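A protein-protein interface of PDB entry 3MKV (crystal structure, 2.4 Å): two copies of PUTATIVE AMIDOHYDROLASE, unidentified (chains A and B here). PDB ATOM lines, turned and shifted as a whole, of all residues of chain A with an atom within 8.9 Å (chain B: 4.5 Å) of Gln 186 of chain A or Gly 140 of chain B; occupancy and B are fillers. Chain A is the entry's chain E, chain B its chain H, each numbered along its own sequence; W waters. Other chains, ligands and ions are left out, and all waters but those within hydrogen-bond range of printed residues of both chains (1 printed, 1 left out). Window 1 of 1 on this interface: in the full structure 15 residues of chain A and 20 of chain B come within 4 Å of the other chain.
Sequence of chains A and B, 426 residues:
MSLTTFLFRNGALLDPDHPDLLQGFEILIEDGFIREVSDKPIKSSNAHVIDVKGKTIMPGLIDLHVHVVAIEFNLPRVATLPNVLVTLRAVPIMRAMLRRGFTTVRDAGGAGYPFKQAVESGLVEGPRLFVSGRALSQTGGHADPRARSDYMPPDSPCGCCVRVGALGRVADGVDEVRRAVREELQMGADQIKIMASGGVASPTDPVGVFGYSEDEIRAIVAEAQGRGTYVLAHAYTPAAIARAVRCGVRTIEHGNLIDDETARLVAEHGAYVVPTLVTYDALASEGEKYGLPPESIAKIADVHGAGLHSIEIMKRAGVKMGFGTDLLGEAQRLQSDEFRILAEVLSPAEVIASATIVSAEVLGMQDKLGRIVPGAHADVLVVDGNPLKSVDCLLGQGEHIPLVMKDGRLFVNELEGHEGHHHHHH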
ATOM      1  N   TYR A 113      18.675   8.679 -18.581  1.00  0.00           N
ATOM      2  CA  TYR A 113      17.828   7.536 -18.242  1.00  0.00           C
ATOM      3  C   TYR A 113      17.684   7.277 -16.732  1.00  0.00           C
ATOM      4  O   TYR A 113      16.585   7.021 -16.247  1.00  0.00           O
ATOM      5  CB  TYR A 113      18.360   6.293 -18.950  1.00  0.00           C
ATOM      6  CG  TYR A 113      17.410   5.124 -18.974  1.00  0.00           C
ATOM      7  CD1 TYR A 113      16.328   5.100 -19.846  1.00  0.00           C
ATOM      8  CD2 TYR A 113      17.607   4.026 -18.142  1.00  0.00           C
ATOM      9  CE1 TYR A 113      15.461   4.016 -19.875  1.00  0.00           C
ATOM     10  CE2 TYR A 113      16.744   2.943 -18.163  1.00  0.00           C
ATOM     11  CZ  TYR A 113      15.675   2.945 -19.029  1.00  0.00           C
ATOM     12  OH  TYR A 113      14.824   1.865 -19.055  1.00  0.00           O
ATOM     13  N   VAL A 162      29.884   9.815 -17.272  1.00  0.00           N
ATOM     14  CA  VAL A 162      29.059  11.002 -17.466  1.00  0.00           C
ATOM     15  C   VAL A 162      28.969  11.779 -16.152  1.00  0.00           C
ATOM     16  O   VAL A 162      28.801  11.188 -15.085  1.00  0.00           O
ATOM     17  CB  VAL A 162      27.633  10.607 -17.920  1.00  0.00           C
ATOM     18  CG1 VAL A 162      26.687  11.788 -17.827  1.00  0.00           C
ATOM     19  CG2 VAL A 162      27.658  10.039 -19.324  1.00  0.00           C
ATOM     20  N   ARG A 169      27.663  17.947 -24.293  1.00  0.00           N
ATOM     21  CA  ARG A 169      28.908  17.253 -24.598  1.00  0.00           C
ATOM     22  C   ARG A 169      29.380  17.730 -25.949  1.00  0.00           C
ATOM     23  O   ARG A 169      28.576  17.919 -26.866  1.00  0.00           O
ATOM     24  CB  ARG A 169      28.722  15.737 -24.621  1.00  0.00           C
ATOM     25  CG  ARG A 169      27.812  15.241 -25.735  1.00  0.00           C
ATOM     26  CD  ARG A 169      27.639  13.733 -25.675  1.00  0.00           C
ATOM     27  NE  ARG A 169      28.843  13.024 -26.092  1.00  0.00           N
ATOM     28  CZ  ARG A 169      28.939  11.700 -26.177  1.00  0.00           C
ATOM     29  NH1 ARG A 169      30.073  11.143 -26.569  1.00  0.00           N
ATOM     30  NH2 ARG A 169      27.902  10.933 -25.873  1.00  0.00           N
ATOM     31  N   ARG A 178      27.978  10.950 -35.086  1.00  0.00           N
ATOM     32  CA  ARG A 178      27.236   9.693 -35.204  1.00  0.00           C
ATOM     33  C   ARG A 178      27.477   8.803 -33.984  1.00  0.00           C
ATOM     34  O   ARG A 178      26.552   8.176 -33.482  1.00  0.00           O
ATOM     35  CB  ARG A 178      27.591   8.935 -36.497  1.00  0.00           C
ATOM     36  CG  ARG A 178      26.847   9.401 -37.771  1.00  0.00           C
ATOM     37  CD  ARG A 178      26.463   8.199 -38.650  1.00  0.00           C
ATOM     38  NE  ARG A 178      26.134   8.526 -40.044  1.00  0.00           N
ATOM     39  CZ  ARG A 178      24.948   8.969 -40.469  1.00  0.00           C
ATOM     40  NH1 ARG A 178      23.964   9.183 -39.603  1.00  0.00           N
ATOM     41  NH2 ARG A 178      24.749   9.213 -41.765  1.00  0.00           N
ATOM     42  N   ARG A 179      28.718   8.751 -33.508  1.00  0.00           N
ATOM     43  CA  ARG A 179      29.035   7.928 -32.343  1.00  0.00           C
ATOM     44  C   ARG A 179      28.396   8.513 -31.086  1.00  0.00           C
ATOM     45  O   ARG A 179      27.868   7.782 -30.245  1.00  0.00           O
ATOM     46  CB  ARG A 179      30.556   7.763 -32.170  1.00  0.00           C
ATOM     47  CG  ARG A 179      30.971   6.778 -31.068  1.00  0.00           C
ATOM     48  CD  ARG A 179      32.438   6.320 -31.199  1.00  0.00           C
ATOM     49  NE  ARG A 179      33.357   7.418 -31.524  1.00  0.00           N
ATOM     50  CZ  ARG A 179      33.989   7.562 -32.693  1.00  0.00           C
ATOM     51  NH1 ARG A 179      33.822   6.671 -33.666  1.00  0.00           N
ATOM     52  NH2 ARG A 179      34.795   8.601 -32.890  1.00  0.00           N
ATOM     53  N   ALA A 180      28.444   9.836 -30.971  1.00  0.00           N
ATOM     54  CA  ALA A 180      27.836  10.535 -29.852  1.00  0.00           C
ATOM     55  C   ALA A 180      26.360  10.155 -29.709  1.00  0.00           C
ATOM     56  O   ALA A 180      25.895   9.804 -28.620  1.00  0.00           O
ATOM     57  CB  ALA A 180      27.994  12.042 -30.024  1.00  0.00           C
ATOM     58  N   VAL A 181      25.624  10.203 -30.815  1.00  0.00           N
ATOM     59  CA  VAL A 181      24.197   9.927 -30.759  1.00  0.00           C
ATOM     60  C   VAL A 181      23.936   8.477 -30.374  1.00  0.00           C
ATOM     61  O   VAL A 181      23.117   8.184 -29.496  1.00  0.00           O
ATOM     62  CB  VAL A 181      23.511  10.281 -32.077  1.00  0.00           C
ATOM     63  CG1 VAL A 181      22.155   9.628 -32.157  1.00  0.00           C
ATOM     64  CG2 VAL A 181      23.377  11.773 -32.178  1.00  0.00           C
ATOM     65  N   ARG A 182      24.661   7.573 -31.018  1.00  0.00           N
ATOM     66  CA  ARG A 182      24.528   6.152 -30.751  1.00  0.00           C
ATOM     67  C   ARG A 182      24.774   5.858 -29.275  1.00  0.00           C
ATOM     68  O   ARG A 182      24.177   4.939 -28.709  1.00  0.00           O
ATOM     69  CB  ARG A 182      25.488   5.362 -31.637  1.00  0.00           C
ATOM     70  CG  ARG A 182      25.103   5.403 -33.116  1.00  0.00           C
ATOM     71  CD  ARG A 182      26.107   4.656 -34.002  1.00  0.00           C
ATOM     72  NE  ARG A 182      25.735   4.784 -35.408  1.00  0.00           N
ATOM     73  CZ  ARG A 182      26.535   4.538 -36.439  1.00  0.00           C
ATOM     74  NH1 ARG A 182      27.784   4.129 -36.253  1.00  0.00           N
ATOM     75  NH2 ARG A 182      26.075   4.705 -37.669  1.00  0.00           N
ATOM     76  N   GLU A 183      25.646   6.645 -28.651  1.00  0.00           N
ATOM     77  CA  GLU A 183      25.945   6.483 -27.232  1.00  0.00           C
ATOM     78  C   GLU A 183      24.802   6.946 -26.342  1.00  0.00           C
ATOM     79  O   GLU A 183      24.408   6.233 -25.424  1.00  0.00           O
ATOM     80  CB  GLU A 183      27.215   7.234 -26.853  1.00  0.00           C
ATOM     81  CG  GLU A 183      28.477   6.470 -27.148  1.00  0.00           C
ATOM     82  CD  GLU A 183      29.710   7.348 -27.082  1.00  0.00           C
ATOM     83  OE1 GLU A 183      29.738   8.289 -26.258  1.00  0.00           O
ATOM     84  OE2 GLU A 183      30.649   7.101 -27.864  1.00  0.00           O
ATOM     85  N   GLU A 184      24.297   8.152 -26.597  1.00  0.00           N
ATOM     86  CA  GLU A 184      23.180   8.682 -25.832  1.00  0.00           C
ATOM     87  C   GLU A 184      21.961   7.767 -25.974  1.00  0.00           C
ATOM     88  O   GLU A 184      21.250   7.508 -24.997  1.00  0.00           O
ATOM     89  CB  GLU A 184      22.843  10.110 -26.273  1.00  0.00           C
ATOM     90  CG  GLU A 184      23.957  11.137 -26.055  1.00  0.00           C
ATOM     91  CD  GLU A 184      24.361  11.291 -24.593  1.00  0.00           C
ATOM     92  OE1 GLU A 184      23.477  11.297 -23.711  1.00  0.00           O
ATOM     93  OE2 GLU A 184      25.568  11.426 -24.324  1.00  0.00           O
ATOM     94  N   LEU A 185      21.729   7.271 -27.189  1.00  0.00           N
ATOM     95  CA  LEU A 185      20.615   6.354 -27.438  1.00  0.00           C
ATOM     96  C   LEU A 185      20.774   5.031 -26.700  1.00  0.00           C
ATOM     97  O   LEU A 185      19.791   4.473 -26.212  1.00  0.00           O
ATOM     98  CB  LEU A 185      20.421   6.106 -28.940  1.00  0.00           C
ATOM     99  CG  LEU A 185      19.978   7.320 -29.761  1.00  0.00           C
ATOM    100  CD1 LEU A 185      19.780   6.949 -31.226  1.00  0.00           C
ATOM    101  CD2 LEU A 185      18.701   7.942 -29.200  1.00  0.00           C
ATOM    102  N   GLN A 186      22.004   4.530 -26.591  1.00  0.00           N
ATOM    103  CA  GLN A 186      22.204   3.257 -25.890  1.00  0.00           C
ATOM    104  C   GLN A 186      22.110   3.442 -24.375  1.00  0.00           C
ATOM    105  O   GLN A 186      21.744   2.520 -23.642  1.00  0.00           O
ATOM    106  CB  GLN A 186      23.512   2.562 -26.302  1.00  0.00           C
ATOM    107  CG  GLN A 186      24.678   2.799 -25.384  1.00  0.00           C
ATOM    108  CD  GLN A 186      24.681   1.875 -24.179  1.00  0.00           C
ATOM    109  OE1 GLN A 186      24.462   0.667 -24.304  1.00  0.00           O
ATOM    110  NE2 GLN A 186      24.947   2.441 -23.001  1.00  0.00           N
ATOM    111  N   MET A 187      22.414   4.641 -23.903  1.00  0.00           N
ATOM    112  CA  MET A 187      22.239   4.927 -22.491  1.00  0.00           C
ATOM    113  C   MET A 187      20.765   5.221 -22.138  1.00  0.00           C
ATOM    114  O   MET A 187      20.437   5.432 -20.974  1.00  0.00           O
ATOM    115  CB  MET A 187      23.193   6.046 -22.030  1.00  0.00           C
ATOM    116  CG  MET A 187      24.642   5.566 -21.780  1.00  0.00           C
ATOM    117  SD  MET A 187      25.803   6.857 -21.253  1.00  0.00           S
ATOM    118  CE  MET A 187      25.870   7.788 -22.762  1.00  0.00           C
ATOM    119  N   GLY A 188      19.886   5.232 -23.141  1.00  0.00           N
ATOM    120  CA  GLY A 188      18.442   5.358 -22.902  1.00  0.00           C
ATOM    121  C   GLY A 188      17.719   6.672 -23.223  1.00  0.00           C
ATOM    122  O   GLY A 188      16.557   6.848 -22.841  1.00  0.00           O
ATOM    123  N   ALA A 189      18.377   7.599 -23.917  1.00  0.00           N
ATOM    124  CA  ALA A 189      17.707   8.844 -24.321  1.00  0.00           C
ATOM    125  C   ALA A 189      16.397   8.595 -25.106  1.00  0.00           C
ATOM    126  O   ALA A 189      16.272   7.606 -25.840  1.00  0.00           O
ATOM    127  CB  ALA A 189      18.656   9.729 -25.133  1.00  0.00           C
ATOM    128  N   ASP A 190      15.432   9.500 -24.959  1.00  0.00           N
ATOM    129  CA  ASP A 190      14.176   9.394 -25.681  1.00  0.00           C
ATOM    130  C   ASP A 190      14.228  10.183 -26.997  1.00  0.00           C
ATOM    131  O   ASP A 190      13.559   9.843 -27.987  1.00  0.00           O
ATOM    132  CB  ASP A 190      13.027   9.884 -24.802  1.00  0.00           C
ATOM    133  CG  ASP A 190      12.909   9.098 -23.491  1.00  0.00           C
ATOM    134  OD1 ASP A 190      12.580   7.891 -23.545  1.00  0.00           O
ATOM    135  OD2 ASP A 190      13.131   9.687 -22.405  1.00  0.00           O
ATOM    136  N   ILE A 192      16.887  13.480 -29.200  1.00  0.00           N
ATOM    137  CA  ILE A 192      18.246  13.997 -29.301  1.00  0.00           C
ATOM    138  C   ILE A 192      18.268  15.502 -29.449  1.00  0.00           C
ATOM    139  O   ILE A 192      17.595  16.065 -30.309  1.00  0.00           O
ATOM    140  CB  ILE A 192      19.044  13.321 -30.454  1.00  0.00           C
ATOM    141  CG1 ILE A 192      19.231  11.821 -30.174  1.00  0.00           C
ATOM    142  CG2 ILE A 192      20.393  13.961 -30.623  1.00  0.00           C
ATOM    143  CD1 ILE A 192      20.086  11.512 -28.941  1.00  0.00           C
ATOM    144  N   ARG A 227      16.343   5.087 -35.046  1.00  0.00           N
ATOM    145  CA  ARG A 227      15.802   4.457 -33.841  1.00  0.00           C
ATOM    146  C   ARG A 227      14.352   4.880 -33.571  1.00  0.00           C
ATOM    147  O   ARG A 227      13.807   4.622 -32.500  1.00  0.00           O
ATOM    148  CB  ARG A 227      16.674   4.773 -32.618  1.00  0.00           C
ATOM    149  CG  ARG A 227      16.608   3.698 -31.528  1.00  0.00           C
ATOM    150  CD  ARG A 227      17.063   4.220 -30.177  1.00  0.00           C
ATOM    151  NE  ARG A 227      17.195   3.150 -29.183  1.00  0.00           N
ATOM    152  CZ  ARG A 227      18.268   2.371 -29.057  1.00  0.00           C
ATOM    153  NH1 ARG A 227      19.309   2.534 -29.863  1.00  0.00           N
ATOM    154  NH2 ARG A 227      18.303   1.428 -28.123  1.00  0.00           N
ATOM    155  N   GLN B 138      27.337  -1.354 -34.924  1.00  0.00           N
ATOM    156  CA  GLN B 138      27.439   0.025 -34.527  1.00  0.00           C
ATOM    157  C   GLN B 138      27.434   0.080 -33.019  1.00  0.00           C
ATOM    158  O   GLN B 138      27.061  -0.886 -32.351  1.00  0.00           O
ATOM    159  CB  GLN B 138      26.278   0.843 -35.103  1.00  0.00           C
ATOM    160  CG  GLN B 138      24.913   0.552 -34.527  1.00  0.00           C
ATOM    161  CD  GLN B 138      23.895   1.652 -34.851  1.00  0.00           C
ATOM    162  OE1 GLN B 138      23.551   1.874 -36.017  1.00  0.00           O
ATOM    163  NE2 GLN B 138      23.410   2.343 -33.816  1.00  0.00           N
ATOM    164  N   THR B 139      27.876   1.199 -32.471  1.00  0.00           N
ATOM    165  CA  THR B 139      27.760   1.382 -31.043  1.00  0.00           C
ATOM    166  C   THR B 139      26.291   1.237 -30.666  1.00  0.00           C
ATOM    167  O   THR B 139      25.421   1.815 -31.310  1.00  0.00           O
ATOM    168  CB  THR B 139      28.283   2.759 -30.617  1.00  0.00           C
ATOM    169  OG1 THR B 139      29.714   2.755 -30.690  1.00  0.00           O
ATOM    170  CG2 THR B 139      27.846   3.085 -29.191  1.00  0.00           C
ATOM    171  N   GLY B 140      26.018   0.454 -29.634  1.00  0.00           N
ATOM    172  CA  GLY B 140      24.646   0.260 -29.171  1.00  0.00           C
ATOM    173  C   GLY B 140      23.885  -0.731 -30.034  1.00  0.00           C
ATOM    174  O   GLY B 140      22.684  -0.926 -29.855  1.00  0.00           O
ATOM    175  N   GLY B 141      24.588  -1.363 -30.970  1.00  0.00           N
ATOM    176  CA  GLY B 141      23.953  -2.292 -31.900  1.00  0.00           C
ATOM    177  C   GLY B 141      23.722  -3.683 -31.327  1.00  0.00           C
ATOM    178  O   GLY B 141      23.909  -3.921 -30.128  1.00  0.00           O
ATOM    179  N   HIS B 142      23.339  -4.610 -32.197  1.00  0.00           N
ATOM    180  CA  HIS B 142      22.956  -5.950 -31.772  1.00  0.00           C
ATOM    181  C   HIS B 142      24.150  -6.769 -31.272  1.00  0.00           C
ATOM    182  O   HIS B 142      23.986  -7.694 -30.481  1.00  0.00           O
ATOM    183  CB  HIS B 142      22.202  -6.673 -32.899  1.00  0.00           C
ATOM    184  CG  HIS B 142      21.746  -8.052 -32.535  1.00  0.00           C
ATOM    185  ND1 HIS B 142      21.033  -8.322 -31.387  1.00  0.00           N
ATOM    186  CD2 HIS B 142      21.900  -9.238 -33.171  1.00  0.00           C
ATOM    187  CE1 HIS B 142      20.773  -9.617 -31.327  1.00  0.00           C
ATOM    188  NE2 HIS B 142      21.285 -10.194 -32.399  1.00  0.00           N
ATOM    189  N   ASP B 144      26.728  -5.298 -29.642  1.00  0.00           N
ATOM    190  CA  ASP B 144      27.371  -4.469 -28.616  1.00  0.00           C
ATOM    191  C   ASP B 144      26.937  -4.928 -27.223  1.00  0.00           C
ATOM    192  O   ASP B 144      25.841  -4.611 -26.774  1.00  0.00           O
ATOM    193  CB  ASP B 144      27.025  -2.991 -28.824  1.00  0.00           C
ATOM    194  CG  ASP B 144      27.684  -2.087 -27.806  1.00  0.00           C
ATOM    195  OD1 ASP B 144      28.233  -2.604 -26.804  1.00  0.00           O
ATOM    196  OD2 ASP B 144      27.649  -0.852 -28.006  1.00  0.00           O
ATOM    197  N   ARG B 146      27.702  -4.288 -24.160  1.00  0.00           N
ATOM    198  CA  ARG B 146      27.731  -3.407 -23.003  1.00  0.00           C
ATOM    199  C   ARG B 146      26.366  -3.147 -22.362  1.00  0.00           C
ATOM    200  O   ARG B 146      25.348  -3.004 -23.044  1.00  0.00           O
ATOM    201  CB  ARG B 146      28.428  -2.100 -23.371  1.00  0.00           C
ATOM    202  CG  ARG B 146      29.923  -2.288 -23.578  1.00  0.00           C
ATOM    203  CD  ARG B 146      30.566  -1.047 -24.134  1.00  0.00           C
ATOM    204  NE  ARG B 146      30.113  -0.788 -25.492  1.00  0.00           N
ATOM    205  CZ  ARG B 146      30.523   0.243 -26.219  1.00  0.00           C
ATOM    206  NH1 ARG B 146      31.400   1.091 -25.697  1.00  0.00           N
ATOM    207  NH2 ARG B 146      30.064   0.419 -27.457  1.00  0.00           N
ATOM    208  N   ALA B 147      26.347  -3.110 -21.036  1.00  0.00           N
ATOM    209  CA  ALA B 147      25.095  -2.924 -20.324  1.00  0.00           C
ATOM    210  C   ALA B 147      24.680  -1.469 -20.453  1.00  0.00           C
ATOM    211  O   ALA B 147      25.437  -0.643 -20.960  1.00  0.00           O
ATOM    212  CB  ALA B 147      25.226  -3.327 -18.857  1.00  0.00           C
ATOM    213  N   ARG B 148      23.501  -1.149 -19.953  1.00  0.00           N
ATOM    214  CA  ARG B 148      23.045   0.217 -19.961  1.00  0.00           C
ATOM    215  C   ARG B 148      23.319   0.812 -18.596  1.00  0.00           C
ATOM    216  O   ARG B 148      22.926   0.263 -17.577  1.00  0.00           O
ATOM    217  CB  ARG B 148      21.561   0.299 -20.285  1.00  0.00           C
ATOM    218  CG  ARG B 148      20.946   1.641 -19.972  1.00  0.00           C
ATOM    219  CD  ARG B 148      19.567   1.766 -20.533  1.00  0.00           C
ATOM    220  NE  ARG B 148      19.595   1.906 -21.973  1.00  0.00           N
ATOM    221  CZ  ARG B 148      18.527   1.825 -22.747  1.00  0.00           C
ATOM    222  NH1 ARG B 148      17.342   1.603 -22.215  1.00  0.00           N
ATOM    223  NH2 ARG B 148      18.644   1.961 -24.050  1.00  0.00           N
ATOM    224  N   MET B 152      30.084   4.649 -20.750  1.00  0.00           N
ATOM    225  CA  MET B 152      30.432   3.695 -21.803  1.00  0.00           C
ATOM    226  C   MET B 152      31.834   3.162 -21.552  1.00  0.00           C
ATOM    227  O   MET B 152      32.817   3.839 -21.859  1.00  0.00           O
ATOM    228  CB  MET B 152      30.417   4.376 -23.184  1.00  0.00           C
ATOM    229  CG  MET B 152      29.139   5.137 -23.535  1.00  0.00           C
ATOM    230  SD  MET B 152      27.756   4.051 -23.920  1.00  0.00           S
ATOM    231  CE  MET B 152      28.526   2.873 -25.035  1.00  0.00           C
ATOM    232  N   THR B 204      20.724  -3.948 -25.006  1.00  0.00           N
ATOM    233  CA  THR B 204      20.092  -2.622 -25.131  1.00  0.00           C
ATOM    234  C   THR B 204      19.213  -2.374 -26.367  1.00  0.00           C
ATOM    235  O   THR B 204      18.181  -1.704 -26.281  1.00  0.00           O
ATOM    236  CB  THR B 204      21.158  -1.498 -25.087  1.00  0.00           C
ATOM    237  OG1 THR B 204      21.929  -1.602 -23.883  1.00  0.00           O
ATOM    238  CG2 THR B 204      20.494  -0.134 -25.151  1.00  0.00           C
ATOM    239  N   ASP B 205      19.633  -2.897 -27.514  1.00  0.00           N
ATOM    240  CA  ASP B 205      19.000  -2.573 -28.791  1.00  0.00           C
ATOM    241  C   ASP B 205      17.619  -3.203 -28.969  1.00  0.00           C
ATOM    242  O   ASP B 205      17.468  -4.420 -28.839  1.00  0.00           O
ATOM    243  CB  ASP B 205      19.911  -3.001 -29.949  1.00  0.00           C
ATOM    244  CG  ASP B 205      20.265  -4.489 -29.898  1.00  0.00           C
ATOM    245  OD1 ASP B 205      20.460  -5.094 -30.977  1.00  0.00           O
ATOM    246  OD2 ASP B 205      20.343  -5.054 -28.781  1.00  0.00           O
HETATM  247  O   HOH W   1      26.184   2.460 -20.839  1.00  0.00           O
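O of Gln 186 of chain A is in hydrogen-bond range of NE of Arg 148 of chain B (2.8 Å).
The side-chain amide nitrogen of Gln 186 of chain A lies within hydrogen-bond range of the side-chain sulfur of Met 152 of chain B, at 3.4 Å.
The side-chain amide oxygen (OE1) of Gln 186 of chain A sits at hydrogen-bond distance from the side-chain hydroxyl (OG1) of Thr 204 of chain B.
The guanidinium group (NH1) of Arg 169 of chain A is in salt-bridge range of the side-chain carboxylate (OE1) of Glu 183 of chain A (2.9 Å).
OD2 of Asp 144 of chain B is in hydrogen-bond range of N of Gly 140 of chain B (2.6 Å).
The guanidinium group (NH2) of Arg 146 of chain B lies within salt-bridge range of the side-chain carboxylate (OD2) of Asp 144 of chain B, at 2.8 Å.
Among the printed residues, pairs that only touch across the chains: Tyr 113 of chain A with Arg 148 of chain B (3.8 Å), Arg 182 of chain A with Gln 138 of chain B (3.6 Å), Arg 182 of chain A with Thr 139 of chain B (3.6 Å), Glu 183 of chain A with Met 152 of chain B (3.9 Å), Leu 185 of chain A with Arg 148 of chain B (3.5 Å), Gln 186 of chain A with Gly 140 of chain B (3.8 Å), Gln 186 of chain A with Arg 146 of chain B (3.98 Å), Gln 186 of chain A with Ala 147 of chain B (3.7 Å), Met 187 of chain A with Arg 148 of chain B (3.5 Å), Gly 188 of chain A with Arg 148 of chain B (3.5 Å) and Arg 227 of chain A with Thr 204 of chain B (3.6 Å).
Of the printed residues of chain B, Gln 186 of chain A touches Gly 140 (3.8 Å), Arg 146 (3.98 Å), Ala 147 (3.7 Å), Arg 148 (2.8 Å), Met 152 (3.4 Å) and Thr 204 (3.3 Å).
Printed residues of chain B within 4 Å of Gly 188 of chain A: Arg 148.
Printed residues of chain A within 4 Å of Gln 138 of chain B: Arg 182.
Printed residues of chain A within 4 Å of Thr 139 of chain B: Arg 182 (3.6 Å).
Gly 140 of chain B touches just one residue of chain A: Gln 186.
No residue of chain A comes within 4 Å of Gly 141 of chain B.
Of the printed residues of chain A, Arg 146 of chain B touches Gln 186 (3.98 Å).
Printed residues of chain A within 4 Å of Thr 204 of chain B: Gln 186 and Arg 227.
The nearest printed residue of chain B that does not touch Met 187 of chain A is Met 152 of chain B (4.1 Å).
Of the 12 printed residues of chain B, 8 touch a printed residue of chain A.
Among the printed residues, 14 pairs touch across the chains.
Among the printed residues, no Asp or Glu carboxylate lies within 4 Å of a Lys or Arg side-chain nitrogen of the other chain.
No position is printed for both chains.
Of the 14 pairs that touch across the chains among the printed residues, none has its exchanged pair printed and touching as well.
Water W1 lies within hydrogen-bond range of NE2 of Gln 186 of chain A (2.5 Å) and O of Ala 147 of chain B (3.2 Å).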
